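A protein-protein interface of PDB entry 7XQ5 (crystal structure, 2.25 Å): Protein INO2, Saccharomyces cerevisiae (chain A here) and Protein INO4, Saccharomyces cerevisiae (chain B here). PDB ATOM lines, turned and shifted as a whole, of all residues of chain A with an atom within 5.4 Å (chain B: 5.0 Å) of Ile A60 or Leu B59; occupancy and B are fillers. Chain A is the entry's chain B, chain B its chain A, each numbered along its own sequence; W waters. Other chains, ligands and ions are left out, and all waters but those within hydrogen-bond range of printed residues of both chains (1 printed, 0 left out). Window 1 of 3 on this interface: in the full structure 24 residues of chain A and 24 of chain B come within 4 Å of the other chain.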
ATOM      1  N   ASN A  55      13.817 -26.472   5.665  1.00  0.00           N
ATOM      2  CA  ASN A  55      14.019 -25.083   5.254  1.00  0.00           C
ATOM      3  C   ASN A  55      12.734 -24.483   4.696  1.00  0.00           C
ATOM      4  O   ASN A  55      12.291 -23.421   5.147  1.00  0.00           O
ATOM      5  CB  ASN A  55      15.133 -24.986   4.214  1.00  0.00           C
ATOM      6  CG  ASN A  55      16.491 -25.351   4.771  1.00  0.00           C
ATOM      7  OD1 ASN A  55      16.704 -25.372   5.992  1.00  0.00           O
ATOM      8  ND2 ASN A  55      17.435 -25.625   3.872  1.00  0.00           N
ATOM      9  N   ASP A  56      12.112 -25.159   3.719  1.00  0.00           N
ATOM     10  CA  ASP A  56      10.890 -24.628   3.119  1.00  0.00           C
ATOM     11  C   ASP A  56       9.815 -24.394   4.170  1.00  0.00           C
ATOM     12  O   ASP A  56       9.116 -23.376   4.132  1.00  0.00           O
ATOM     13  CB  ASP A  56      10.364 -25.565   2.026  1.00  0.00           C
ATOM     14  CG  ASP A  56      11.108 -25.411   0.699  1.00  0.00           C
ATOM     15  OD1 ASP A  56      12.309 -25.044   0.704  1.00  0.00           O
ATOM     16  OD2 ASP A  56      10.474 -25.658  -0.355  1.00  0.00           O
ATOM     17  N   ILE A  57       9.660 -25.320   5.117  1.00  0.00           N
ATOM     18  CA  ILE A  57       8.667 -25.116   6.168  1.00  0.00           C
ATOM     19  C   ILE A  57       8.974 -23.850   6.947  1.00  0.00           C
ATOM     20  O   ILE A  57       8.121 -22.963   7.079  1.00  0.00           O
ATOM     21  CB  ILE A  57       8.593 -26.334   7.098  1.00  0.00           C
ATOM     22  CG1 ILE A  57       8.083 -27.537   6.318  1.00  0.00           C
ATOM     23  CG2 ILE A  57       7.671 -26.022   8.275  1.00  0.00           C
ATOM     24  CD1 ILE A  57       7.918 -28.778   7.167  1.00  0.00           C
ATOM     25  N   LYS A  58      10.199 -23.739   7.471  1.00  0.00           N
ATOM     26  CA  LYS A  58      10.562 -22.549   8.236  1.00  0.00           C
ATOM     27  C   LYS A  58      10.409 -21.294   7.392  1.00  0.00           C
ATOM     28  O   LYS A  58       9.867 -20.284   7.854  1.00  0.00           O
ATOM     29  CB  LYS A  58      11.994 -22.663   8.761  1.00  0.00           C
ATOM     30  CG  LYS A  58      12.202 -23.634   9.927  1.00  0.00           C
ATOM     31  CD  LYS A  58      13.681 -23.646  10.323  1.00  0.00           C
ATOM     32  CE  LYS A  58      13.969 -24.590  11.481  1.00  0.00           C
ATOM     33  NZ  LYS A  58      15.311 -25.255  11.337  1.00  0.00           N
ATOM     34  N   SER A  59      10.852 -21.351   6.138  1.00  0.00           N
ATOM     35  CA  SER A  59      10.843 -20.160   5.300  1.00  0.00           C
ATOM     36  C   SER A  59       9.422 -19.635   5.093  1.00  0.00           C
ATOM     37  O   SER A  59       9.188 -18.422   5.136  1.00  0.00           O
ATOM     38  CB  SER A  59      11.517 -20.475   3.969  1.00  0.00           C
ATOM     39  OG  SER A  59      11.585 -19.326   3.153  1.00  0.00           O
ATOM     40  N   ILE A  60       8.453 -20.533   4.912  1.00  0.00           N
ATOM     41  CA  ILE A  60       7.101 -20.064   4.639  1.00  0.00           C
ATOM     42  C   ILE A  60       6.377 -19.670   5.924  1.00  0.00           C
ATOM     43  O   ILE A  60       5.532 -18.770   5.900  1.00  0.00           O
ATOM     44  CB  ILE A  60       6.311 -21.117   3.844  1.00  0.00           C
ATOM     45  CG1 ILE A  60       4.898 -20.622   3.548  1.00  0.00           C
ATOM     46  CG2 ILE A  60       6.200 -22.391   4.611  1.00  0.00           C
ATOM     47  CD1 ILE A  60       4.843 -19.568   2.481  1.00  0.00           C
ATOM     48  N   ARG A  61       6.675 -20.320   7.055  1.00  0.00           N
ATOM     49  CA  ARG A  61       6.143 -19.850   8.334  1.00  0.00           C
ATOM     50  C   ARG A  61       6.526 -18.399   8.578  1.00  0.00           C
ATOM     51  O   ARG A  61       5.692 -17.581   8.981  1.00  0.00           O
ATOM     52  CB  ARG A  61       6.670 -20.696   9.480  1.00  0.00           C
ATOM     53  CG  ARG A  61       6.272 -22.124   9.467  1.00  0.00           C
ATOM     54  CD  ARG A  61       7.230 -22.860  10.393  1.00  0.00           C
ATOM     55  NE  ARG A  61       7.384 -22.146  11.653  1.00  0.00           N
ATOM     56  CZ  ARG A  61       6.556 -22.294  12.673  1.00  0.00           C
ATOM     57  NH1 ARG A  61       5.555 -23.157  12.622  1.00  0.00           N
ATOM     58  NH2 ARG A  61       6.733 -21.555  13.765  1.00  0.00           N
ATOM     59  N   SER A  62       7.796 -18.071   8.348  1.00  0.00           N
ATOM     60  CA  SER A  62       8.258 -16.706   8.550  1.00  0.00           C
ATOM     61  C   SER A  62       7.498 -15.744   7.654  1.00  0.00           C
ATOM     62  O   SER A  62       6.883 -14.783   8.134  1.00  0.00           O
ATOM     63  CB  SER A  62       9.756 -16.630   8.281  1.00  0.00           C
ATOM     64  OG  SER A  62      10.401 -17.708   8.924  1.00  0.00           O
ATOM     65  N   ALA A  63       7.518 -16.007   6.339  1.00  0.00           N
ATOM     66  CA  ALA A  63       6.783 -15.170   5.390  1.00  0.00           C
ATOM     67  C   ALA A  63       5.357 -14.918   5.863  1.00  0.00           C
ATOM     68  O   ALA A  63       4.870 -13.784   5.815  1.00  0.00           O
ATOM     69  CB  ALA A  63       6.795 -15.814   4.004  1.00  0.00           C
ATOM     70  N   ASN A  64       4.690 -15.952   6.374  1.00  0.00           N
ATOM     71  CA  ASN A  64       3.323 -15.782   6.850  1.00  0.00           C
ATOM     72  C   ASN A  64       3.262 -14.869   8.072  1.00  0.00           C
ATOM     73  O   ASN A  64       2.335 -14.059   8.199  1.00  0.00           O
ATOM     74  CB  ASN A  64       2.697 -17.141   7.164  1.00  0.00           C
ATOM     75  CG  ASN A  64       2.435 -17.964   5.915  1.00  0.00           C
ATOM     76  OD1 ASN A  64       2.552 -17.462   4.798  1.00  0.00           O
ATOM     77  ND2 ASN A  64       2.085 -19.234   6.096  1.00  0.00           N
ATOM     78  N   GLU A  65       4.224 -14.994   8.991  1.00  0.00           N
ATOM     79  CA  GLU A  65       4.223 -14.109  10.154  1.00  0.00           C
ATOM     80  C   GLU A  65       4.467 -12.668   9.734  1.00  0.00           C
ATOM     81  O   GLU A  65       3.772 -11.758  10.197  1.00  0.00           O
ATOM     82  CB  GLU A  65       5.264 -14.566  11.174  1.00  0.00           C
ATOM     83  CG  GLU A  65       5.054 -15.994  11.664  1.00  0.00           C
ATOM     84  CD  GLU A  65       6.011 -16.385  12.782  1.00  0.00           C
ATOM     85  OE1 GLU A  65       6.396 -15.478  13.564  1.00  0.00           O
ATOM     86  OE2 GLU A  65       6.371 -17.591  12.874  1.00  0.00           O
ATOM     87  N   TYR B  55       1.188 -30.144   5.597  1.00  0.00           N
ATOM     88  CA  TYR B  55       1.486 -28.892   6.292  1.00  0.00           C
ATOM     89  C   TYR B  55       1.995 -27.832   5.325  1.00  0.00           C
ATOM     90  O   TYR B  55       1.564 -26.674   5.382  1.00  0.00           O
ATOM     91  CB  TYR B  55       2.490 -29.128   7.426  1.00  0.00           C
ATOM     92  CG  TYR B  55       2.673 -27.929   8.340  1.00  0.00           C
ATOM     93  CD1 TYR B  55       1.578 -27.243   8.846  1.00  0.00           C
ATOM     94  CD2 TYR B  55       3.943 -27.498   8.714  1.00  0.00           C
ATOM     95  CE1 TYR B  55       1.737 -26.146   9.668  1.00  0.00           C
ATOM     96  CE2 TYR B  55       4.116 -26.401   9.554  1.00  0.00           C
ATOM     97  CZ  TYR B  55       3.005 -25.728  10.025  1.00  0.00           C
ATOM     98  OH  TYR B  55       3.161 -24.636  10.850  1.00  0.00           O
ATOM     99  N   LEU B  56       2.905 -28.209   4.424  1.00  0.00           N
ATOM    100  CA  LEU B  56       3.347 -27.286   3.384  1.00  0.00           C
ATOM    101  C   LEU B  56       2.168 -26.712   2.619  1.00  0.00           C
ATOM    102  O   LEU B  56       2.090 -25.501   2.395  1.00  0.00           O
ATOM    103  CB  LEU B  56       4.287 -27.993   2.412  1.00  0.00           C
ATOM    104  CG  LEU B  56       5.776 -27.920   2.708  1.00  0.00           C
ATOM    105  CD1 LEU B  56       6.520 -28.655   1.606  1.00  0.00           C
ATOM    106  CD2 LEU B  56       6.219 -26.468   2.798  1.00  0.00           C
ATOM    107  N   SER B  57       1.245 -27.576   2.187  1.00  0.00           N
ATOM    108  CA  SER B  57       0.109 -27.091   1.409  1.00  0.00           C
ATOM    109  C   SER B  57      -0.689 -26.067   2.189  1.00  0.00           C
ATOM    110  O   SER B  57      -1.090 -25.033   1.642  1.00  0.00           O
ATOM    111  CB  SER B  57      -0.806 -28.236   1.004  1.00  0.00           C
ATOM    112  OG  SER B  57      -1.850 -27.719   0.199  1.00  0.00           O
ATOM    113  N   TRP B  58      -0.941 -26.351   3.471  1.00  0.00           N
ATOM    114  CA  TRP B  58      -1.687 -25.421   4.309  1.00  0.00           C
ATOM    115  C   TRP B  58      -0.922 -24.121   4.495  1.00  0.00           C
ATOM    116  O   TRP B  58      -1.517 -23.042   4.494  1.00  0.00           O
ATOM    117  CB  TRP B  58      -1.985 -26.087   5.643  1.00  0.00           C
ATOM    118  CG  TRP B  58      -2.792 -25.288   6.574  1.00  0.00           C
ATOM    119  CD1 TRP B  58      -4.138 -25.340   6.736  1.00  0.00           C
ATOM    120  CD2 TRP B  58      -2.307 -24.335   7.519  1.00  0.00           C
ATOM    121  NE1 TRP B  58      -4.530 -24.464   7.717  1.00  0.00           N
ATOM    122  CE2 TRP B  58      -3.419 -23.830   8.211  1.00  0.00           C
ATOM    123  CE3 TRP B  58      -1.038 -23.848   7.838  1.00  0.00           C
ATOM    124  CZ2 TRP B  58      -3.305 -22.865   9.204  1.00  0.00           C
ATOM    125  CZ3 TRP B  58      -0.925 -22.883   8.828  1.00  0.00           C
ATOM    126  CH2 TRP B  58      -2.052 -22.403   9.498  1.00  0.00           C
ATOM    127  N   LEU B  59       0.406 -24.196   4.626  1.00  0.00           N
ATOM    128  CA  LEU B  59       1.185 -22.978   4.818  1.00  0.00           C
ATOM    129  C   LEU B  59       1.112 -22.089   3.588  1.00  0.00           C
ATOM    130  O   LEU B  59       0.938 -20.871   3.707  1.00  0.00           O
ATOM    131  CB  LEU B  59       2.637 -23.317   5.157  1.00  0.00           C
ATOM    132  CG  LEU B  59       2.903 -23.783   6.593  1.00  0.00           C
ATOM    133  CD1 LEU B  59       4.257 -24.431   6.719  1.00  0.00           C
ATOM    134  CD2 LEU B  59       2.809 -22.608   7.546  1.00  0.00           C
ATOM    135  N   TYR B  60       1.234 -22.679   2.395  1.00  0.00           N
ATOM    136  CA  TYR B  60       1.058 -21.895   1.176  1.00  0.00           C
ATOM    137  C   TYR B  60      -0.359 -21.348   1.075  1.00  0.00           C
ATOM    138  O   TYR B  60      -0.552 -20.191   0.695  1.00  0.00           O
ATOM    139  CB  TYR B  60       1.400 -22.736  -0.058  1.00  0.00           C
ATOM    140  CG  TYR B  60       2.882 -22.913  -0.269  1.00  0.00           C
ATOM    141  CD1 TYR B  60       3.685 -21.830  -0.598  1.00  0.00           C
ATOM    142  CD2 TYR B  60       3.485 -24.149  -0.109  1.00  0.00           C
ATOM    143  CE1 TYR B  60       5.043 -21.973  -0.785  1.00  0.00           C
ATOM    144  CE2 TYR B  60       4.852 -24.308  -0.299  1.00  0.00           C
ATOM    145  CZ  TYR B  60       5.622 -23.215  -0.635  1.00  0.00           C
ATOM    146  OH  TYR B  60       6.974 -23.358  -0.831  1.00  0.00           O
ATOM    147  N   GLU B  61      -1.363 -22.165   1.408  1.00  0.00           N
ATOM    148  CA  GLU B  61      -2.742 -21.685   1.389  1.00  0.00           C
ATOM    149  C   GLU B  61      -2.904 -20.484   2.306  1.00  0.00           C
ATOM    150  O   GLU B  61      -3.476 -19.459   1.915  1.00  0.00           O
ATOM    151  CB  GLU B  61      -3.704 -22.802   1.801  1.00  0.00           C
ATOM    152  CG  GLU B  61      -3.958 -23.850   0.738  1.00  0.00           C
ATOM    153  CD  GLU B  61      -4.723 -25.047   1.279  1.00  0.00           C
ATOM    154  OE1 GLU B  61      -5.295 -24.911   2.395  1.00  0.00           O
ATOM    155  OE2 GLU B  61      -4.739 -26.118   0.599  1.00  0.00           O
ATOM    156  N   ARG B  62      -2.397 -20.591   3.533  1.00  0.00           N
ATOM    157  CA  ARG B  62      -2.447 -19.457   4.443  1.00  0.00           C
ATOM    158  C   ARG B  62      -1.781 -18.240   3.825  1.00  0.00           C
ATOM    159  O   ARG B  62      -2.303 -17.122   3.923  1.00  0.00           O
ATOM    160  CB  ARG B  62      -1.781 -19.816   5.765  1.00  0.00           C
ATOM    161  CG  ARG B  62      -1.685 -18.645   6.727  1.00  0.00           C
ATOM    162  CD  ARG B  62      -1.377 -19.100   8.154  1.00  0.00           C
ATOM    163  NE  ARG B  62      -0.807 -18.023   8.956  1.00  0.00           N
ATOM    164  CZ  ARG B  62      -1.506 -17.026   9.484  1.00  0.00           C
ATOM    165  NH1 ARG B  62      -2.820 -16.944   9.329  1.00  0.00           N
ATOM    166  NH2 ARG B  62      -0.869 -16.081  10.176  1.00  0.00           N
ATOM    167  N   ASN B  63      -0.639 -18.443   3.165  1.00  0.00           N
ATOM    168  CA  ASN B  63       0.060 -17.334   2.528  1.00  0.00           C
ATOM    169  C   ASN B  63      -0.830 -16.645   1.497  1.00  0.00           C
ATOM    170  O   ASN B  63      -0.914 -15.410   1.458  1.00  0.00           O
ATOM    171  CB  ASN B  63       1.349 -17.843   1.889  1.00  0.00           C
ATOM    172  CG  ASN B  63       2.253 -16.724   1.447  1.00  0.00           C
ATOM    173  OD1 ASN B  63       1.992 -16.066   0.446  1.00  0.00           O
ATOM    174  ND2 ASN B  63       3.331 -16.503   2.186  1.00  0.00           N
HETATM  175  O   HOH W   1       1.640 -19.707   9.247  1.00  0.00           O
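OH of Tyr B55 lies within hydrogen-bond range of NH1 of Arg A61 (3.3 Å).
The side-chain amide nitrogen (ND2) of Asn A64 is in hydrogen-bond range of the backbone carbonyl oxygen (O) of Leu B59, 3.1 Å away.
The side-chain amide nitrogen (ND2) of Asn B63 is in hydrogen-bond range of the side-chain amide oxygen (OD1) of Asn A64.
The backbone carbonyl oxygen of Ile A60 sits close to the side-chain amide oxygen of Asn A64 (3.4 Å).
Among the printed residues, pairs that only touch across the chains: Ile A57 with Tyr B55 (3.8 Å), Ile A60 with Leu B59 (3.5 Å), Ile A60 with Tyr B60 (3.99 Å), Ile A60 with Asn B63 (3.4 Å), Arg A61 with Leu B59 (3.99 Å), Ala A63 with Asn B63 (3.97 Å) and Asn A64 with Arg B62 (3.9 Å).
Printed residues of chain A within 4 Å of Leu B59: Ile A60, Arg A61 and Asn A64.
Of the printed residues of chain A, Tyr B55 touches Ile A57 and Arg A61.
Printed residues of chain B within 4 Å of Asn A64: Leu B59, Arg B62 and Asn B63.
Ser A62 touches none of the printed residues of chain B.
Of the 9 printed residues of chain B, 5 touch a printed residue of chain A.
Printed residues of chain B that touch a printed residue of chain A: Tyr B55, Leu B59, Tyr B60, Arg B62 and Asn B63.
Hydrophobic or aromatic side chains of chain B within 4 Å of the printed part of chain A: Tyr B55, Leu B59 and Tyr B60.
Of the 11 printed residues of chain A, 5 touch a printed residue of chain B.
Printed residues of chain A that touch a printed residue of chain B: Ile A57, Ile A60, Arg A61, Ala A63 and Asn A64.
Hydrophobic or aromatic side chains of chain A within 4 Å of the printed part of chain B: Ile A57, Ile A60 and Ala A63.
Among the printed residues, 10 pairs touch across the chains.
Water W1 bridges the guanidinium group (NE) of Arg B62 (3.0 Å) and the side-chain amide nitrogen (ND2) of Asn A64 (3.2 Å).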
